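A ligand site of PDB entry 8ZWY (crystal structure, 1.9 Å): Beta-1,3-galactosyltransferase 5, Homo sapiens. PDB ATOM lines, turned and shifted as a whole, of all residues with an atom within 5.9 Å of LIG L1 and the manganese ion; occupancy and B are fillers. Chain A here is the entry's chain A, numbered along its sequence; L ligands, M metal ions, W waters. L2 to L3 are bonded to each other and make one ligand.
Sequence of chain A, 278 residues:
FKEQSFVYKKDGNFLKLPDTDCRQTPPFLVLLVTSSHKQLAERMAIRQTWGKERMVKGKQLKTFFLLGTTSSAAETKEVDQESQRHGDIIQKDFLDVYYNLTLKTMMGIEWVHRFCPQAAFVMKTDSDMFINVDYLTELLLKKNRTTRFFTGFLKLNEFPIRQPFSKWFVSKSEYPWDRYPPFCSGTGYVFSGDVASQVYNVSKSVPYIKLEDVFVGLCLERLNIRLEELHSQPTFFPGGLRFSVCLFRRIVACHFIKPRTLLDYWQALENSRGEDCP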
ATOM      1  N   VAL A  33      17.854 -34.132  11.732  1.00  0.00           N
ATOM      2  CA  VAL A  33      18.369 -32.792  12.090  1.00  0.00           C
ATOM      3  C   VAL A  33      19.805 -32.586  11.561  1.00  0.00           C
ATOM      4  O   VAL A  33      20.707 -33.328  11.933  1.00  0.00           O
ATOM      5  CB  VAL A  33      18.301 -32.491  13.605  1.00  0.00           C
ATOM      6  CG1 VAL A  33      18.698 -31.062  13.916  1.00  0.00           C
ATOM      7  CG2 VAL A  33      16.958 -32.853  14.210  1.00  0.00           C
ATOM      8  N   THR A  34      19.983 -31.518  10.795  1.00  0.00           N
ATOM      9  CA  THR A  34      21.305 -31.168  10.282  1.00  0.00           C
ATOM     10  C   THR A  34      22.013 -30.308  11.313  1.00  0.00           C
ATOM     11  O   THR A  34      21.400 -29.420  11.904  1.00  0.00           O
ATOM     12  CB  THR A  34      21.181 -30.480   8.914  1.00  0.00           C
ATOM     13  OG1 THR A  34      20.359 -29.355   9.133  1.00  0.00           O
ATOM     14  CG2 THR A  34      20.568 -31.376   7.858  1.00  0.00           C
ATOM     15  N   SER A  35      23.271 -30.612  11.533  1.00  0.00           N
ATOM     16  CA  SER A  35      24.108 -29.793  12.439  1.00  0.00           C
ATOM     17  C   SER A  35      25.575 -30.067  12.070  1.00  0.00           C
ATOM     18  O   SER A  35      25.849 -31.182  11.632  1.00  0.00           O
ATOM     19  CB  SER A  35      23.815 -30.144  13.879  1.00  0.00           C
ATOM     20  OG  SER A  35      24.486 -31.307  14.333  1.00  0.00           O
ATOM     21  N   SER A  36      26.458 -29.101  12.293  1.00  0.00           N
ATOM     22  CA  SER A  36      27.871 -29.388  12.072  1.00  0.00           C
ATOM     23  C   SER A  36      28.528 -29.923  13.344  1.00  0.00           C
ATOM     24  O   SER A  36      28.010 -29.787  14.453  1.00  0.00           O
ATOM     25  CB  SER A  36      28.602 -28.161  11.541  1.00  0.00           C
ATOM     26  OG  SER A  36      28.613 -27.056  12.420  1.00  0.00           O
ATOM     27  N   GLN A  39      28.558 -27.989  16.707  1.00  0.00           N
ATOM     28  CA  GLN A  39      27.298 -27.534  17.253  1.00  0.00           C
ATOM     29  C   GLN A  39      26.748 -28.522  18.267  1.00  0.00           C
ATOM     30  O   GLN A  39      25.580 -28.918  18.194  1.00  0.00           O
ATOM     31  CB  GLN A  39      26.305 -27.285  16.114  1.00  0.00           C
ATOM     32  CG  GLN A  39      26.620 -26.035  15.263  1.00  0.00           C
ATOM     33  CD  GLN A  39      25.599 -25.725  14.160  1.00  0.00           C
ATOM     34  OE1 GLN A  39      25.409 -26.502  13.246  1.00  0.00           O
ATOM     35  NE2 GLN A  39      24.978 -24.557  14.237  1.00  0.00           N
ATOM     36  N   LEU A  66      22.142 -35.721  11.467  1.00  0.00           N
ATOM     37  CA  LEU A  66      22.923 -36.003  10.245  1.00  0.00           C
ATOM     38  C   LEU A  66      24.277 -35.299  10.356  1.00  0.00           C
ATOM     39  O   LEU A  66      24.323 -34.084  10.515  1.00  0.00           O
ATOM     40  CB  LEU A  66      22.182 -35.536   9.000  1.00  0.00           C
ATOM     41  CG  LEU A  66      20.700 -35.929   8.904  1.00  0.00           C
ATOM     42  CD1 LEU A  66      20.111 -35.399   7.616  1.00  0.00           C
ATOM     43  CD2 LEU A  66      20.542 -37.428   9.002  1.00  0.00           C
ATOM     44  N   ASP A  96      31.921 -32.285   5.928  1.00  0.00           N
ATOM     45  CA  ASP A  96      30.733 -31.578   6.459  1.00  0.00           C
ATOM     46  C   ASP A  96      30.909 -30.055   6.323  1.00  0.00           C
ATOM     47  O   ASP A  96      31.429 -29.453   7.252  1.00  0.00           O
ATOM     48  CB  ASP A  96      30.447 -32.092   7.856  1.00  0.00           C
ATOM     49  CG  ASP A  96      29.024 -31.862   8.333  1.00  0.00           C
ATOM     50  OD1 ASP A  96      28.335 -31.104   7.651  1.00  0.00           O
ATOM     51  OD2 ASP A  96      28.622 -32.460   9.341  1.00  0.00           O
ATOM     52  N   VAL A  97      30.474 -29.489   5.203  1.00  0.00           N
ATOM     53  CA  VAL A  97      30.551 -28.028   4.933  1.00  0.00           C
ATOM     54  C   VAL A  97      29.221 -27.553   4.312  1.00  0.00           C
ATOM     55  O   VAL A  97      28.496 -28.388   3.805  1.00  0.00           O
ATOM     56  CB  VAL A  97      31.735 -27.696   3.989  1.00  0.00           C
ATOM     57  CG1 VAL A  97      33.070 -27.901   4.678  1.00  0.00           C
ATOM     58  CG2 VAL A  97      31.644 -28.480   2.686  1.00  0.00           C
ATOM     59  N   TYR A  98      28.939 -26.258   4.386  1.00  0.00           N
ATOM     60  CA  TYR A  98      27.652 -25.705   3.873  1.00  0.00           C
ATOM     61  C   TYR A  98      27.390 -26.188   2.428  1.00  0.00           C
ATOM     62  O   TYR A  98      26.290 -26.668   2.194  1.00  0.00           O
ATOM     63  CB  TYR A  98      27.551 -24.184   3.993  1.00  0.00           C
ATOM     64  CG  TYR A  98      26.109 -23.689   3.863  1.00  0.00           C
ATOM     65  CD1 TYR A  98      25.279 -23.591   4.966  1.00  0.00           C
ATOM     66  CD2 TYR A  98      25.594 -23.352   2.623  1.00  0.00           C
ATOM     67  CE1 TYR A  98      23.974 -23.150   4.836  1.00  0.00           C
ATOM     68  CE2 TYR A  98      24.284 -22.912   2.479  1.00  0.00           C
ATOM     69  CZ  TYR A  98      23.467 -22.824   3.593  1.00  0.00           C
ATOM     70  OH  TYR A  98      22.190 -22.392   3.439  1.00  0.00           O
ATOM     71  N   LEU A 101      25.791 -29.701   1.947  1.00  0.00           N
ATOM     72  CA  LEU A 101      24.458 -29.980   2.557  1.00  0.00           C
ATOM     73  C   LEU A 101      23.596 -30.906   1.661  1.00  0.00           C
ATOM     74  O   LEU A 101      22.790 -31.642   2.191  1.00  0.00           O
ATOM     75  CB  LEU A 101      23.803 -28.640   2.866  1.00  0.00           C
ATOM     76  CG  LEU A 101      24.256 -27.971   4.161  1.00  0.00           C
ATOM     77  CD1 LEU A 101      23.610 -26.621   4.376  1.00  0.00           C
ATOM     78  CD2 LEU A 101      24.028 -28.886   5.348  1.00  0.00           C
ATOM     79  N   LYS A 104      24.488 -34.289   2.657  1.00  0.00           N
ATOM     80  CA  LYS A 104      23.930 -34.570   3.999  1.00  0.00           C
ATOM     81  C   LYS A 104      22.451 -34.965   3.842  1.00  0.00           C
ATOM     82  O   LYS A 104      22.058 -35.977   4.395  1.00  0.00           O
ATOM     83  CB  LYS A 104      24.048 -33.369   4.938  1.00  0.00           C
ATOM     84  CG  LYS A 104      23.591 -33.647   6.356  1.00  0.00           C
ATOM     85  CD  LYS A 104      24.068 -32.595   7.336  1.00  0.00           C
ATOM     86  CE  LYS A 104      25.541 -32.641   7.550  1.00  0.00           C
ATOM     87  NZ  LYS A 104      25.876 -32.085   8.858  1.00  0.00           N
ATOM     88  N   THR A 125      15.112 -31.064   9.109  1.00  0.00           N
ATOM     89  CA  THR A 125      15.135 -29.728   9.718  1.00  0.00           C
ATOM     90  C   THR A 125      16.528 -29.215  10.071  1.00  0.00           C
ATOM     91  O   THR A 125      17.453 -30.010  10.182  1.00  0.00           O
ATOM     92  CB  THR A 125      14.225 -29.652  10.956  1.00  0.00           C
ATOM     93  OG1 THR A 125      14.120 -28.297  11.377  1.00  0.00           O
ATOM     94  CG2 THR A 125      14.727 -30.506  12.104  1.00  0.00           C
ATOM     95  N   ASP A 126      16.621 -27.903  10.220  1.00  0.00           N
ATOM     96  CA  ASP A 126      17.853 -27.220  10.671  1.00  0.00           C
ATOM     97  C   ASP A 126      17.968 -27.357  12.190  1.00  0.00           C
ATOM     98  O   ASP A 126      16.976 -27.728  12.821  1.00  0.00           O
ATOM     99  CB  ASP A 126      17.728 -25.736  10.419  1.00  0.00           C
ATOM    100  CG  ASP A 126      18.239 -25.163   9.103  1.00  0.00           C
ATOM    101  OD1 ASP A 126      18.096 -25.788   8.063  1.00  0.00           O
ATOM    102  OD2 ASP A 126      18.711 -24.025   9.114  1.00  0.00           O
ATOM    103  N   SER A 127      19.131 -27.016  12.736  1.00  0.00           N
ATOM    104  CA  SER A 127      19.385 -27.070  14.192  1.00  0.00           C
ATOM    105  C   SER A 127      18.901 -25.774  14.872  1.00  0.00           C
ATOM    106  O   SER A 127      18.652 -25.836  16.073  1.00  0.00           O
ATOM    107  CB  SER A 127      20.881 -27.269  14.424  1.00  0.00           C
ATOM    108  OG  SER A 127      21.661 -26.399  13.623  1.00  0.00           O
ATOM    109  N   ASP A 128      18.800 -24.668  14.143  1.00  0.00           N
ATOM    110  CA  ASP A 128      18.433 -23.344  14.757  1.00  0.00           C
ATOM    111  C   ASP A 128      16.917 -23.172  14.616  1.00  0.00           C
ATOM    112  O   ASP A 128      16.468 -22.160  14.078  1.00  0.00           O
ATOM    113  CB  ASP A 128      19.242 -22.207  14.174  1.00  0.00           C
ATOM    114  CG  ASP A 128      19.148 -22.073  12.662  1.00  0.00           C
ATOM    115  OD1 ASP A 128      18.804 -23.065  11.992  1.00  0.00           O
ATOM    116  OD2 ASP A 128      19.416 -20.974  12.177  1.00  0.00           O
ATOM    117  N   MET A 129      16.198 -24.167  15.119  1.00  0.00           N
ATOM    118  CA  MET A 129      14.747 -24.178  14.863  1.00  0.00           C
ATOM    119  C   MET A 129      13.940 -24.578  16.100  1.00  0.00           C
ATOM    120  O   MET A 129      14.493 -25.200  17.001  1.00  0.00           O
ATOM    121  CB  MET A 129      14.430 -25.236  13.805  1.00  0.00           C
ATOM    122  CG  MET A 129      15.043 -25.008  12.440  1.00  0.00           C
ATOM    123  SD  MET A 129      14.100 -23.781  11.521  1.00  0.00           S
ATOM    124  CE  MET A 129      12.531 -24.663  11.393  1.00  0.00           C
ATOM    125  N   LYS A 167      25.372 -16.013   0.028  1.00  0.00           N
ATOM    126  CA  LYS A 167      25.461 -17.406   0.535  1.00  0.00           C
ATOM    127  C   LYS A 167      24.811 -18.386  -0.456  1.00  0.00           C
ATOM    128  O   LYS A 167      25.325 -19.482  -0.627  1.00  0.00           O
ATOM    129  CB  LYS A 167      24.658 -17.450   1.826  1.00  0.00           C
ATOM    130  CG  LYS A 167      24.818 -18.672   2.709  1.00  0.00           C
ATOM    131  CD  LYS A 167      23.829 -18.654   3.867  1.00  0.00           C
ATOM    132  CE  LYS A 167      24.051 -19.774   4.817  1.00  0.00           C
ATOM    133  NZ  LYS A 167      23.993 -19.325   6.213  1.00  0.00           N
ATOM    134  N   TRP A 168      23.707 -17.994  -1.068  1.00  0.00           N
ATOM    135  CA  TRP A 168      22.960 -18.919  -1.961  1.00  0.00           C
ATOM    136  C   TRP A 168      23.292 -18.657  -3.438  1.00  0.00           C
ATOM    137  O   TRP A 168      22.564 -19.108  -4.319  1.00  0.00           O
ATOM    138  CB  TRP A 168      21.471 -18.789  -1.656  1.00  0.00           C
ATOM    139  CG  TRP A 168      21.129 -19.123  -0.230  1.00  0.00           C
ATOM    140  CD1 TRP A 168      21.482 -20.235   0.471  1.00  0.00           C
ATOM    141  CD2 TRP A 168      20.346 -18.309   0.676  1.00  0.00           C
ATOM    142  NE1 TRP A 168      20.992 -20.160   1.747  1.00  0.00           N
ATOM    143  CE2 TRP A 168      20.279 -19.001   1.894  1.00  0.00           C
ATOM    144  CE3 TRP A 168      19.700 -17.069   0.553  1.00  0.00           C
ATOM    145  CZ2 TRP A 168      19.602 -18.501   2.996  1.00  0.00           C
ATOM    146  CZ3 TRP A 168      19.027 -16.580   1.638  1.00  0.00           C
ATOM    147  CH2 TRP A 168      18.972 -17.288   2.846  1.00  0.00           C
ATOM    148  N   THR A 187      14.868 -25.036   5.760  1.00  0.00           N
ATOM    149  CA  THR A 187      14.795 -24.860   7.226  1.00  0.00           C
ATOM    150  C   THR A 187      14.032 -26.001   7.876  1.00  0.00           C
ATOM    151  O   THR A 187      14.364 -26.381   8.997  1.00  0.00           O
ATOM    152  CB  THR A 187      14.150 -23.507   7.554  1.00  0.00           C
ATOM    153  OG1 THR A 187      12.881 -23.368   6.943  1.00  0.00           O
ATOM    154  CG2 THR A 187      15.056 -22.348   7.145  1.00  0.00           C
ATOM    155  N   HIS A 255      12.194 -20.561  12.546  1.00  0.00           N
ATOM    156  CA  HIS A 255      13.650 -20.505  12.338  1.00  0.00           C
ATOM    157  C   HIS A 255      14.271 -19.399  13.202  1.00  0.00           C
ATOM    158  O   HIS A 255      13.536 -18.753  13.952  1.00  0.00           O
ATOM    159  CB  HIS A 255      13.860 -20.277  10.839  1.00  0.00           C
ATOM    160  CG  HIS A 255      15.224 -20.265  10.320  1.00  0.00           C
ATOM    161  ND1 HIS A 255      15.596 -19.294   9.424  1.00  0.00           N
ATOM    162  CD2 HIS A 255      16.276 -21.036  10.512  1.00  0.00           C
ATOM    163  CE1 HIS A 255      16.852 -19.482   9.086  1.00  0.00           C
ATOM    164  NE2 HIS A 255      17.265 -20.530   9.730  1.00  0.00           N
ATOM    165  N   PHE A 256      15.597 -19.228  13.114  1.00  0.00           N
ATOM    166  CA  PHE A 256      16.301 -18.144  13.852  1.00  0.00           C
ATOM    167  C   PHE A 256      16.179 -18.339  15.363  1.00  0.00           C
ATOM    168  O   PHE A 256      16.002 -17.355  16.077  1.00  0.00           O
ATOM    169  CB  PHE A 256      15.800 -16.782  13.360  1.00  0.00           C
ATOM    170  CG  PHE A 256      16.153 -16.488  11.902  1.00  0.00           C
ATOM    171  CD1 PHE A 256      17.417 -16.767  11.418  1.00  0.00           C
ATOM    172  CD2 PHE A 256      15.214 -15.957  11.040  1.00  0.00           C
ATOM    173  CE1 PHE A 256      17.742 -16.501  10.101  1.00  0.00           C
ATOM    174  CE2 PHE A 256      15.538 -15.692   9.723  1.00  0.00           C
ATOM    175  CZ  PHE A 256      16.798 -15.970   9.263  1.00  0.00           C
HETATM  176  N1  LIG L   1      25.003 -27.161   8.712  1.00  0.00           N
HETATM  177  C1  LIG L   1      25.621 -28.427   8.682  1.00  0.00           C
HETATM  178  N2  LIG L   1      26.948 -28.420   8.335  1.00  0.00           N
HETATM  179  C2  LIG L   1      27.716 -27.321   8.010  1.00  0.00           C
HETATM  180  C3  LIG L   1      27.013 -26.060   8.034  1.00  0.00           C
HETATM  181  C4  LIG L   1      25.712 -26.022   8.406  1.00  0.00           C
HETATM  182  O1  LIG L   1      25.050 -29.468   8.992  1.00  0.00           O
HETATM  183  O2  LIG L   1      28.899 -27.482   7.697  1.00  0.00           O
HETATM  184  C5  LIG L   1      23.597 -27.088   9.119  1.00  0.00           C
HETATM  185  C6  LIG L   1      23.299 -26.055  10.197  1.00  0.00           C
HETATM  186  O3  LIG L   1      23.572 -26.553  11.490  1.00  0.00           O
HETATM  187  C7  LIG L   1      21.809 -25.843   9.969  1.00  0.00           C
HETATM  188  C8  LIG L   1      21.731 -25.876   8.433  1.00  0.00           C
HETATM  189  O4  LIG L   1      22.873 -26.655   8.007  1.00  0.00           O
HETATM  190  O5  LIG L   1      21.069 -26.888  10.581  1.00  0.00           O
HETATM  191  C9  LIG L   1      21.770 -24.537   7.735  1.00  0.00           C
HETATM  192  O6  LIG L   1      22.850 -23.780   8.332  1.00  0.00           O
HETATM  193  P1  LIG L   1      22.620 -22.309   8.849  1.00  0.00           P
HETATM  194  O7  LIG L   1      23.895 -21.838   9.405  1.00  0.00           O
HETATM  195  O8  LIG L   1      21.449 -22.249   9.812  1.00  0.00           O
HETATM  196  O9  LIG L   1      22.213 -21.482   7.594  1.00  0.00           O
HETATM  197  P2  LIG L   1      20.809 -21.003   7.015  1.00  0.00           P
HETATM  198  O10 LIG L   1      19.578 -20.919   8.224  1.00  0.00           O
HETATM  199  O11 LIG L   1      20.623 -21.964   5.804  1.00  0.00           O
HETATM  200  O12 LIG L   1      21.153 -19.679   6.358  1.00  0.00           O
HETATM  201  C1  LG2 L   2      15.171 -14.642   0.452  1.00  0.00           C
HETATM  202  C2  LG2 L   2      15.045 -16.104   0.874  1.00  0.00           C
HETATM  203  C3  LG2 L   2      15.689 -17.024  -0.154  1.00  0.00           C
HETATM  204  C4  LG2 L   2      15.188 -16.708  -1.541  1.00  0.00           C
HETATM  205  C5  LG2 L   2      15.458 -15.248  -1.835  1.00  0.00           C
HETATM  206  C6  LG2 L   2      14.999 -14.821  -3.215  1.00  0.00           C
HETATM  207  C7  LG2 L   2      14.593 -12.489   1.186  1.00  0.00           C
HETATM  208  O1  LG2 L   2      14.405 -13.885   1.340  1.00  0.00           O
HETATM  209  O2  LG2 L   2      15.641 -16.314   2.145  1.00  0.00           O
HETATM  210  O3  LG2 L   2      15.422 -18.378   0.176  1.00  0.00           O
HETATM  211  O4  LG2 L   2      13.804 -16.960  -1.600  1.00  0.00           O
HETATM  212  O5  LG2 L   2      14.739 -14.449  -0.876  1.00  0.00           O
HETATM  213  O6  LG2 L   2      15.265 -13.460  -3.462  1.00  0.00           O
HETATM  214  C1  LG3 L   3      16.515 -19.214  -0.019  1.00  0.00           C
HETATM  215  C2  LG3 L   3      16.413 -20.401   0.932  1.00  0.00           C
HETATM  216  C3  LG3 L   3      17.558 -21.373   0.662  1.00  0.00           C
HETATM  217  C4  LG3 L   3      17.543 -21.775  -0.801  1.00  0.00           C
HETATM  218  C5  LG3 L   3      17.703 -20.496  -1.614  1.00  0.00           C
HETATM  219  C6  LG3 L   3      17.764 -20.714  -3.103  1.00  0.00           C
HETATM  220  C7  LG3 L   3      15.378 -20.049   3.129  1.00  0.00           C
HETATM  221  C8  LG3 L   3      15.445 -19.246   4.386  1.00  0.00           C
HETATM  222  N1  LG3 L   3      16.424 -19.956   2.311  1.00  0.00           N
HETATM  223  O1  LG3 L   3      17.472 -22.497   1.520  1.00  0.00           O
HETATM  224  O2  LG3 L   3      18.618 -22.668  -1.060  1.00  0.00           O
HETATM  225  O3  LG3 L   3      16.564 -19.663  -1.366  1.00  0.00           O
HETATM  226  O4  LG3 L   3      17.922 -19.471  -3.762  1.00  0.00           O
HETATM  227  O5  LG3 L   3      14.412 -20.747   2.863  1.00  0.00           O
HETATM  228 MN    MN M   1      19.311 -21.798   9.806  1.00  0.00          MN
HETATM  229  O   HOH W   1      18.172 -20.141   5.667  1.00  0.00           O
HETATM  230  O   HOH W   2      22.369 -22.168  12.112  1.00  0.00           O
HETATM  231  O   HOH W   3      18.735 -24.535   5.312  1.00  0.00           O
HETATM  232  O   HOH W   4      31.552 -27.030   8.778  1.00  0.00           O
HETATM  233  O   HOH W   5      25.529 -23.282  11.026  1.00  0.00           O
HETATM  234  O   HOH W   6      20.136 -18.884  10.217  1.00  0.00           O
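Within 4 Å of the manganese ion: Asp 126, Asp 128 and His 255.
N of Ser 36 touches O1 of LIG L1 (3.6 Å).
CA of Val 97 touches O2 of LIG L1, at 3.3 Å.
Leu 101 touches LIG L1.
CZ2 of Trp 168 touches O12 of LIG L1 (3.9 Å).
Hydrophobic or aromatic side chains within 4 Å of LIG L1: Tyr 98, Leu 101, Trp 168 and His 255.
Of the 21 residues printed, 15 come within 4 Å of LIG L1.
The manganese ion is bound by O10 of LIG L1 (1.8 Å).
The manganese ion is bound by O8 of LIG L1 (2.2 Å).
OD2 of Asp 126 binds the manganese ion.
The manganese ion is bound by a ring nitrogen (NE2) of His 255 (2.4 Å).
OD2 of Asp 128 is bound to the manganese ion (2.5 Å).
OD1 of Asp 128 is bound to the manganese ion (2.6 Å).
O of Ser 35 sits at hydrogen-bond distance from NZ of Lys 104.
The backbone carbonyl oxygen of Asp 128 is in hydrogen-bond range of the backbone NH of Phe 256 (3.2 Å).
NZ of Lys 104 lies within salt-bridge range of OD2 of Asp 96, at 2.8 Å.
The backbone carbonyl oxygen of Thr 187 sits at hydrogen-bond distance from the backbone NH of Asp 126 (3.0 Å).
OE1 of Gln 39 is in hydrogen-bond range of N of Ser 36 (3.0 Å).
The backbone NH of Thr 34 lies within hydrogen-bond range of the backbone carbonyl oxygen of Thr 125, at 3.0 Å.
NZ of Lys 104 is in hydrogen-bond range of O of Leu 66, at 3.0 Å.
The backbone carbonyl oxygen (O) of Thr 34 sits close to the backbone NH (N) of Ser 127 (3.4 Å).
An oxygen (O3) of LIG L1 lies within hydrogen-bond range of the side-chain hydroxyl (OG) of Ser 127 (2.9 Å).
The side-chain amino group of Lys 167 lies within salt-bridge range of an oxygen (O12) of LIG L1 (2.9 Å).
NZ of Lys 104 lies within hydrogen-bond range of O1 of LIG L1 (2.7 Å).
The side-chain amide oxygen (OE1) of Gln 39 lies within hydrogen-bond range of an oxygen (O3) of LIG L1 (2.5 Å).
An oxygen (O5) of LIG L1 sits at hydrogen-bond distance from the backbone carbonyl oxygen (O) of Thr 34.
OH of Tyr 98 lies within hydrogen-bond range of O11 of LIG L1 (2.9 Å).
OD1 of Asp 96 is in hydrogen-bond range of N2 of LIG L1, at 3.1 Å.
An oxygen (O5) of LIG L1 sits at hydrogen-bond distance from the side-chain hydroxyl (OG1) of Thr 34 (2.9 Å).
The backbone NH (N) of Ser 127 sits at hydrogen-bond distance from an oxygen (O5) of LIG L1 (2.9 Å).
N of Ser 35 lies close to O1 of LIG L1 (3.3 Å).
Water W5 bridges an oxygen (O7) of LIG L1 and the side-chain amide nitrogen of Gln 39.
Water W4 lies within hydrogen-bond range of the backbone carbonyl oxygen (O) of Asp 96 (2.9 Å) and an oxygen (O2) of LIG L1 (2.9 Å).
Water W3 bridges OD1 of Asp 126 and O11 of LIG L1.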
